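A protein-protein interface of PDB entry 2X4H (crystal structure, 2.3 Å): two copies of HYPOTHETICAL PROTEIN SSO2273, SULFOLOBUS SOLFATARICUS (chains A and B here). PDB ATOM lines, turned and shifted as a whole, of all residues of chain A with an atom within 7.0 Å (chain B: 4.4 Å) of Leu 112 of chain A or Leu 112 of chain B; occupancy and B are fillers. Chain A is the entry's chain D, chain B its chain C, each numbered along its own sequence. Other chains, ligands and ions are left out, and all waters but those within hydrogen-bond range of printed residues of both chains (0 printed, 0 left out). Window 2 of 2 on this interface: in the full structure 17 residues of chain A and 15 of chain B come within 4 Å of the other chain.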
ATOM      1  N   LEU A  11     -26.879 -10.155  -6.389  1.00  0.00           N
ATOM      2  CA  LEU A  11     -28.155 -10.508  -5.705  1.00  0.00           C
ATOM      3  C   LEU A  11     -27.854 -11.415  -4.521  1.00  0.00           C
ATOM      4  O   LEU A  11     -27.186 -12.424  -4.696  1.00  0.00           O
ATOM      5  CB  LEU A  11     -29.095 -11.236  -6.672  1.00  0.00           C
ATOM      6  CG  LEU A  11     -30.527 -11.544  -6.199  1.00  0.00           C
ATOM      7  CD1 LEU A  11     -31.355 -10.282  -6.054  1.00  0.00           C
ATOM      8  CD2 LEU A  11     -31.236 -12.488  -7.160  1.00  0.00           C
ATOM      9  N   SER A  12     -28.346 -11.069  -3.330  1.00  0.00           N
ATOM     10  CA  SER A  12     -28.227 -11.947  -2.157  1.00  0.00           C
ATOM     11  C   SER A  12     -29.352 -12.983  -2.136  1.00  0.00           C
ATOM     12  O   SER A  12     -30.325 -12.866  -2.883  1.00  0.00           O
ATOM     13  CB  SER A  12     -28.237 -11.126  -0.866  1.00  0.00           C
ATOM     14  OG  SER A  12     -29.440 -10.406  -0.734  1.00  0.00           O
ATOM     15  N   LEU A  81     -29.933 -16.874 -10.495  1.00  0.00           N
ATOM     16  CA  LEU A  81     -29.565 -17.571  -9.251  1.00  0.00           C
ATOM     17  C   LEU A  81     -30.002 -19.041  -9.335  1.00  0.00           C
ATOM     18  O   LEU A  81     -29.281 -19.921  -8.908  1.00  0.00           O
ATOM     19  CB  LEU A  81     -30.161 -16.865  -8.031  1.00  0.00           C
ATOM     20  CG  LEU A  81     -29.612 -17.206  -6.653  1.00  0.00           C
ATOM     21  CD1 LEU A  81     -28.079 -17.198  -6.669  1.00  0.00           C
ATOM     22  CD2 LEU A  81     -30.150 -16.240  -5.597  1.00  0.00           C
ATOM     23  N   TYR A 105     -26.697 -27.927   0.464  1.00  0.00           N
ATOM     24  CA  TYR A 105     -25.308 -27.391   0.473  1.00  0.00           C
ATOM     25  C   TYR A 105     -25.167 -26.247  -0.547  1.00  0.00           C
ATOM     26  O   TYR A 105     -24.633 -25.185  -0.236  1.00  0.00           O
ATOM     27  CB  TYR A 105     -24.271 -28.449   0.107  1.00  0.00           C
ATOM     28  CG  TYR A 105     -23.839 -29.425   1.187  1.00  0.00           C
ATOM     29  CD1 TYR A 105     -24.035 -29.194   2.552  1.00  0.00           C
ATOM     30  CD2 TYR A 105     -23.156 -30.576   0.813  1.00  0.00           C
ATOM     31  CE1 TYR A 105     -23.591 -30.128   3.496  1.00  0.00           C
ATOM     32  CE2 TYR A 105     -22.721 -31.495   1.734  1.00  0.00           C
ATOM     33  CZ  TYR A 105     -22.938 -31.291   3.058  1.00  0.00           C
ATOM     34  OH  TYR A 105     -22.460 -32.282   3.914  1.00  0.00           O
ATOM     35  N   GLN A 108     -25.860 -22.619   0.457  1.00  0.00           N
ATOM     36  CA  GLN A 108     -24.904 -21.931   1.318  1.00  0.00           C
ATOM     37  C   GLN A 108     -23.943 -21.005   0.550  1.00  0.00           C
ATOM     38  O   GLN A 108     -23.413 -20.069   1.139  1.00  0.00           O
ATOM     39  CB  GLN A 108     -24.102 -22.945   2.161  1.00  0.00           C
ATOM     40  CG  GLN A 108     -24.987 -23.763   3.109  1.00  0.00           C
ATOM     41  CD  GLN A 108     -24.218 -24.676   4.049  1.00  0.00           C
ATOM     42  OE1 GLN A 108     -23.210 -24.279   4.632  1.00  0.00           O
ATOM     43  NE2 GLN A 108     -24.711 -25.904   4.226  1.00  0.00           N
ATOM     44  N   PHE A 109     -23.698 -21.264  -0.737  1.00  0.00           N
ATOM     45  CA  PHE A 109     -22.732 -20.447  -1.506  1.00  0.00           C
ATOM     46  C   PHE A 109     -23.015 -20.208  -3.003  1.00  0.00           C
ATOM     47  O   PHE A 109     -22.244 -19.514  -3.674  1.00  0.00           O
ATOM     48  CB  PHE A 109     -21.324 -21.051  -1.373  1.00  0.00           C
ATOM     49  CG  PHE A 109     -21.207 -22.449  -1.919  1.00  0.00           C
ATOM     50  CD1 PHE A 109     -20.821 -22.665  -3.223  1.00  0.00           C
ATOM     51  CD2 PHE A 109     -21.483 -23.550  -1.116  1.00  0.00           C
ATOM     52  CE1 PHE A 109     -20.709 -23.945  -3.723  1.00  0.00           C
ATOM     53  CE2 PHE A 109     -21.384 -24.838  -1.620  1.00  0.00           C
ATOM     54  CZ  PHE A 109     -20.995 -25.031  -2.925  1.00  0.00           C
ATOM     55  N   ASP A 110     -24.108 -20.746  -3.533  1.00  0.00           N
ATOM     56  CA  ASP A 110     -24.344 -20.634  -4.963  1.00  0.00           C
ATOM     57  C   ASP A 110     -24.420 -19.190  -5.454  1.00  0.00           C
ATOM     58  O   ASP A 110     -24.003 -18.885  -6.565  1.00  0.00           O
ATOM     59  CB  ASP A 110     -25.577 -21.442  -5.413  1.00  0.00           C
ATOM     60  CG  ASP A 110     -26.849 -21.126  -4.633  1.00  0.00           C
ATOM     61  OD1 ASP A 110     -26.907 -20.166  -3.830  1.00  0.00           O
ATOM     62  OD2 ASP A 110     -27.818 -21.890  -4.831  1.00  0.00           O
ATOM     63  N   TYR A 111     -24.944 -18.318  -4.612  1.00  0.00           N
ATOM     64  CA  TYR A 111     -25.135 -16.905  -4.922  1.00  0.00           C
ATOM     65  C   TYR A 111     -23.846 -16.086  -4.858  1.00  0.00           C
ATOM     66  O   TYR A 111     -23.809 -14.965  -5.346  1.00  0.00           O
ATOM     67  CB  TYR A 111     -26.188 -16.308  -3.981  1.00  0.00           C
ATOM     68  CG  TYR A 111     -25.844 -16.290  -2.492  1.00  0.00           C
ATOM     69  CD1 TYR A 111     -25.527 -15.095  -1.838  1.00  0.00           C
ATOM     70  CD2 TYR A 111     -25.880 -17.463  -1.715  1.00  0.00           C
ATOM     71  CE1 TYR A 111     -25.235 -15.071  -0.454  1.00  0.00           C
ATOM     72  CE2 TYR A 111     -25.581 -17.439  -0.330  1.00  0.00           C
ATOM     73  CZ  TYR A 111     -25.258 -16.249   0.277  1.00  0.00           C
ATOM     74  OH  TYR A 111     -24.971 -16.239   1.629  1.00  0.00           O
ATOM     75  N   LEU A 112     -22.804 -16.640  -4.235  1.00  0.00           N
ATOM     76  CA  LEU A 112     -21.544 -15.917  -4.012  1.00  0.00           C
ATOM     77  C   LEU A 112     -20.467 -16.317  -4.995  1.00  0.00           C
ATOM     78  O   LEU A 112     -19.349 -15.805  -4.926  1.00  0.00           O
ATOM     79  CB  LEU A 112     -21.036 -16.159  -2.606  1.00  0.00           C
ATOM     80  CG  LEU A 112     -21.894 -15.536  -1.518  1.00  0.00           C
ATOM     81  CD1 LEU A 112     -21.228 -15.811  -0.197  1.00  0.00           C
ATOM     82  CD2 LEU A 112     -22.110 -14.031  -1.734  1.00  0.00           C
ATOM     83  N   ILE A 113     -20.805 -17.225  -5.910  1.00  0.00           N
ATOM     84  CA  ILE A 113     -19.850 -17.732  -6.861  1.00  0.00           C
ATOM     85  C   ILE A 113     -19.809 -16.823  -8.078  1.00  0.00           C
ATOM     86  O   ILE A 113     -20.839 -16.544  -8.686  1.00  0.00           O
ATOM     87  CB  ILE A 113     -20.176 -19.176  -7.277  1.00  0.00           C
ATOM     88  CG1 ILE A 113     -19.902 -20.120  -6.103  1.00  0.00           C
ATOM     89  CG2 ILE A 113     -19.292 -19.612  -8.445  1.00  0.00           C
ATOM     90  CD1 ILE A 113     -20.447 -21.500  -6.332  1.00  0.00           C
ATOM     91  N   PRO A 114     -18.607 -16.352  -8.444  1.00  0.00           N
ATOM     92  CA  PRO A 114     -18.521 -15.502  -9.635  1.00  0.00           C
ATOM     93  C   PRO A 114     -19.121 -16.127 -10.905  1.00  0.00           C
ATOM     94  O   PRO A 114     -18.938 -17.321 -11.177  1.00  0.00           O
ATOM     95  CB  PRO A 114     -17.015 -15.259  -9.805  1.00  0.00           C
ATOM     96  CG  PRO A 114     -16.336 -15.949  -8.681  1.00  0.00           C
ATOM     97  CD  PRO A 114     -17.345 -16.393  -7.694  1.00  0.00           C
ATOM     98  N   GLU A 115     -19.790 -15.281 -11.675  1.00  0.00           N
ATOM     99  CA  GLU A 115     -20.498 -15.645 -12.905  1.00  0.00           C
ATOM    100  C   GLU A 115     -19.655 -16.535 -13.805  1.00  0.00           C
ATOM    101  O   GLU A 115     -20.135 -17.530 -14.357  1.00  0.00           O
ATOM    102  CB  GLU A 115     -20.917 -14.373 -13.707  1.00  0.00           C
ATOM    103  CG  GLU A 115     -21.168 -13.082 -12.892  1.00  0.00           C
ATOM    104  CD  GLU A 115     -21.574 -11.868 -13.749  1.00  0.00           C
ATOM    105  OE1 GLU A 115     -21.599 -11.960 -14.996  1.00  0.00           O
ATOM    106  OE2 GLU A 115     -21.851 -10.801 -13.160  1.00  0.00           O
ATOM    107  N   GLN B 108     -13.013 -15.939  -2.893  1.00  0.00           N
ATOM    108  CA  GLN B 108     -14.363 -15.409  -2.680  1.00  0.00           C
ATOM    109  C   GLN B 108     -15.388 -16.412  -2.135  1.00  0.00           C
ATOM    110  O   GLN B 108     -16.450 -16.006  -1.715  1.00  0.00           O
ATOM    111  CB  GLN B 108     -14.892 -14.768  -3.978  1.00  0.00           C
ATOM    112  CG  GLN B 108     -14.131 -13.510  -4.371  1.00  0.00           C
ATOM    113  CD  GLN B 108     -14.562 -12.944  -5.699  1.00  0.00           C
ATOM    114  OE1 GLN B 108     -15.757 -12.768  -5.956  1.00  0.00           O
ATOM    115  NE2 GLN B 108     -13.582 -12.633  -6.557  1.00  0.00           N
ATOM    116  N   PHE B 109     -15.108 -17.710  -2.152  1.00  0.00           N
ATOM    117  CA  PHE B 109     -16.076 -18.682  -1.616  1.00  0.00           C
ATOM    118  C   PHE B 109     -15.499 -19.965  -0.996  1.00  0.00           C
ATOM    119  O   PHE B 109     -16.242 -20.718  -0.360  1.00  0.00           O
ATOM    120  CB  PHE B 109     -17.112 -19.056  -2.694  1.00  0.00           C
ATOM    121  CG  PHE B 109     -16.537 -19.752  -3.890  1.00  0.00           C
ATOM    122  CD1 PHE B 109     -16.591 -21.141  -4.003  1.00  0.00           C
ATOM    123  CD2 PHE B 109     -15.971 -19.018  -4.934  1.00  0.00           C
ATOM    124  CE1 PHE B 109     -16.051 -21.802  -5.125  1.00  0.00           C
ATOM    125  CE2 PHE B 109     -15.431 -19.661  -6.050  1.00  0.00           C
ATOM    126  CZ  PHE B 109     -15.471 -21.059  -6.146  1.00  0.00           C
ATOM    127  N   ASP B 110     -14.201 -20.220  -1.179  1.00  0.00           N
ATOM    128  CA  ASP B 110     -13.569 -21.407  -0.594  1.00  0.00           C
ATOM    129  C   ASP B 110     -13.947 -21.641   0.854  1.00  0.00           C
ATOM    130  O   ASP B 110     -14.283 -22.753   1.202  1.00  0.00           O
ATOM    131  CB  ASP B 110     -12.039 -21.411  -0.757  1.00  0.00           C
ATOM    132  CG  ASP B 110     -11.368 -20.133  -0.304  1.00  0.00           C
ATOM    133  OD1 ASP B 110     -11.963 -19.330   0.475  1.00  0.00           O
ATOM    134  OD2 ASP B 110     -10.202 -19.923  -0.728  1.00  0.00           O
ATOM    135  N   TYR B 111     -13.915 -20.589   1.670  1.00  0.00           N
ATOM    136  CA  TYR B 111     -14.197 -20.665   3.116  1.00  0.00           C
ATOM    137  C   TYR B 111     -15.661 -20.988   3.464  1.00  0.00           C
ATOM    138  O   TYR B 111     -15.971 -21.284   4.604  1.00  0.00           O
ATOM    139  CB  TYR B 111     -13.789 -19.345   3.813  1.00  0.00           C
ATOM    140  CG  TYR B 111     -14.641 -18.136   3.410  1.00  0.00           C
ATOM    141  CD1 TYR B 111     -15.656 -17.671   4.247  1.00  0.00           C
ATOM    142  CD2 TYR B 111     -14.441 -17.473   2.194  1.00  0.00           C
ATOM    143  CE1 TYR B 111     -16.455 -16.586   3.883  1.00  0.00           C
ATOM    144  CE2 TYR B 111     -15.238 -16.396   1.817  1.00  0.00           C
ATOM    145  CZ  TYR B 111     -16.238 -15.953   2.677  1.00  0.00           C
ATOM    146  OH  TYR B 111     -17.030 -14.890   2.333  1.00  0.00           O
ATOM    147  N   LEU B 112     -16.562 -20.934   2.481  1.00  0.00           N
ATOM    148  CA  LEU B 112     -17.979 -21.262   2.711  1.00  0.00           C
ATOM    149  C   LEU B 112     -18.322 -22.719   2.366  1.00  0.00           C
ATOM    150  O   LEU B 112     -19.396 -23.187   2.715  1.00  0.00           O
ATOM    151  CB  LEU B 112     -18.879 -20.287   1.922  1.00  0.00           C
ATOM    152  CG  LEU B 112     -18.811 -18.881   2.541  1.00  0.00           C
ATOM    153  CD1 LEU B 112     -19.077 -17.784   1.528  1.00  0.00           C
ATOM    154  CD2 LEU B 112     -19.743 -18.735   3.774  1.00  0.00           C
ATOM    155  N   ILE B 113     -17.428 -23.435   1.685  1.00  0.00           N
ATOM    156  CA  ILE B 113     -17.759 -24.784   1.218  1.00  0.00           C
ATOM    157  C   ILE B 113     -17.652 -25.771   2.383  1.00  0.00           C
ATOM    158  O   ILE B 113     -16.635 -25.796   3.054  1.00  0.00           O
ATOM    159  CB  ILE B 113     -16.839 -25.267   0.053  1.00  0.00           C
ATOM    160  CG1 ILE B 113     -16.863 -24.291  -1.136  1.00  0.00           C
ATOM    161  CG2 ILE B 113     -17.280 -26.620  -0.454  1.00  0.00           C
ATOM    162  CD1 ILE B 113     -18.222 -24.041  -1.689  1.00  0.00           C
ATOM    163  N   PRO B 114     -18.711 -26.566   2.635  1.00  0.00           N
ATOM    164  CA  PRO B 114     -18.689 -27.656   3.624  1.00  0.00           C
ATOM    165  C   PRO B 114     -17.670 -28.778   3.344  1.00  0.00           C
ATOM    166  O   PRO B 114     -17.345 -29.076   2.178  1.00  0.00           O
ATOM    167  CB  PRO B 114     -20.096 -28.234   3.542  1.00  0.00           C
ATOM    168  CG  PRO B 114     -20.942 -27.120   3.015  1.00  0.00           C
ATOM    169  CD  PRO B 114     -20.067 -26.346   2.098  1.00  0.00           C
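Of the 7 printed residues of chain B, 3 touch a printed residue of chain A. Hydrophobic or aromatic side chains of chain B that line the printed part of chain A: Leu 112, Ile 113 and Pro 114. Hydrophobic or aromatic side chains of chain A that line the printed part of chain B: Tyr 105, Phe 109 and Leu 112. Along chain A the printed residues that touch a printed residue of chain B span positions 105 to 112. Among the printed residues, 4 pairs touch across the chains.
Pro 114 of chain B touches Tyr 105 of chain A. OE1 of Gln 108 of chain A touches CG of Pro 114 of chain B, 3.98 Å away. Ile 113 of chain B touches Phe 109 of chain A (CD1 to CZ, 3.2 Å). CD1 of Leu 112 of chain B touches CD1 of Leu 112 of chain A, 3.4 Å away.
Gln 108 of chain A touches Pro 114 of chain B, but with the chains exchanged Pro 114 of chain A does not touch Gln 108 of chain B (4.2 Å). Phe 109 of chain A touches Ile 113 of chain B, but with the chains exchanged Ile 113 of chain A does not touch Phe 109 of chain B (4.04 Å). Leu 112 of chain A touches its own counterpart, Leu 112 of chain B. Of the 4 pairs that touch across the chains among the printed residues, 1 has its exchanged pair printed and touching as well.
Leu 11 of chain A touches none of the printed residues of chain B. Of the printed residues of chain B, Tyr 105 of chain A touches Pro 114 (3.8 Å). Of the printed residues of chain B, Gln 108 of chain A touches Pro 114. Leu 112 of chain A touches one residue of chain B. Leu 112 of chain B touches one residue of chain A. The nearest residue of chain B that does not touch Leu 112 of chain A is Gln 108 of chain B (4.3 Å). The nearest printed residue of chain B that does not touch Tyr 105 of chain A is Leu 112 of chain B (6.3 Å).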
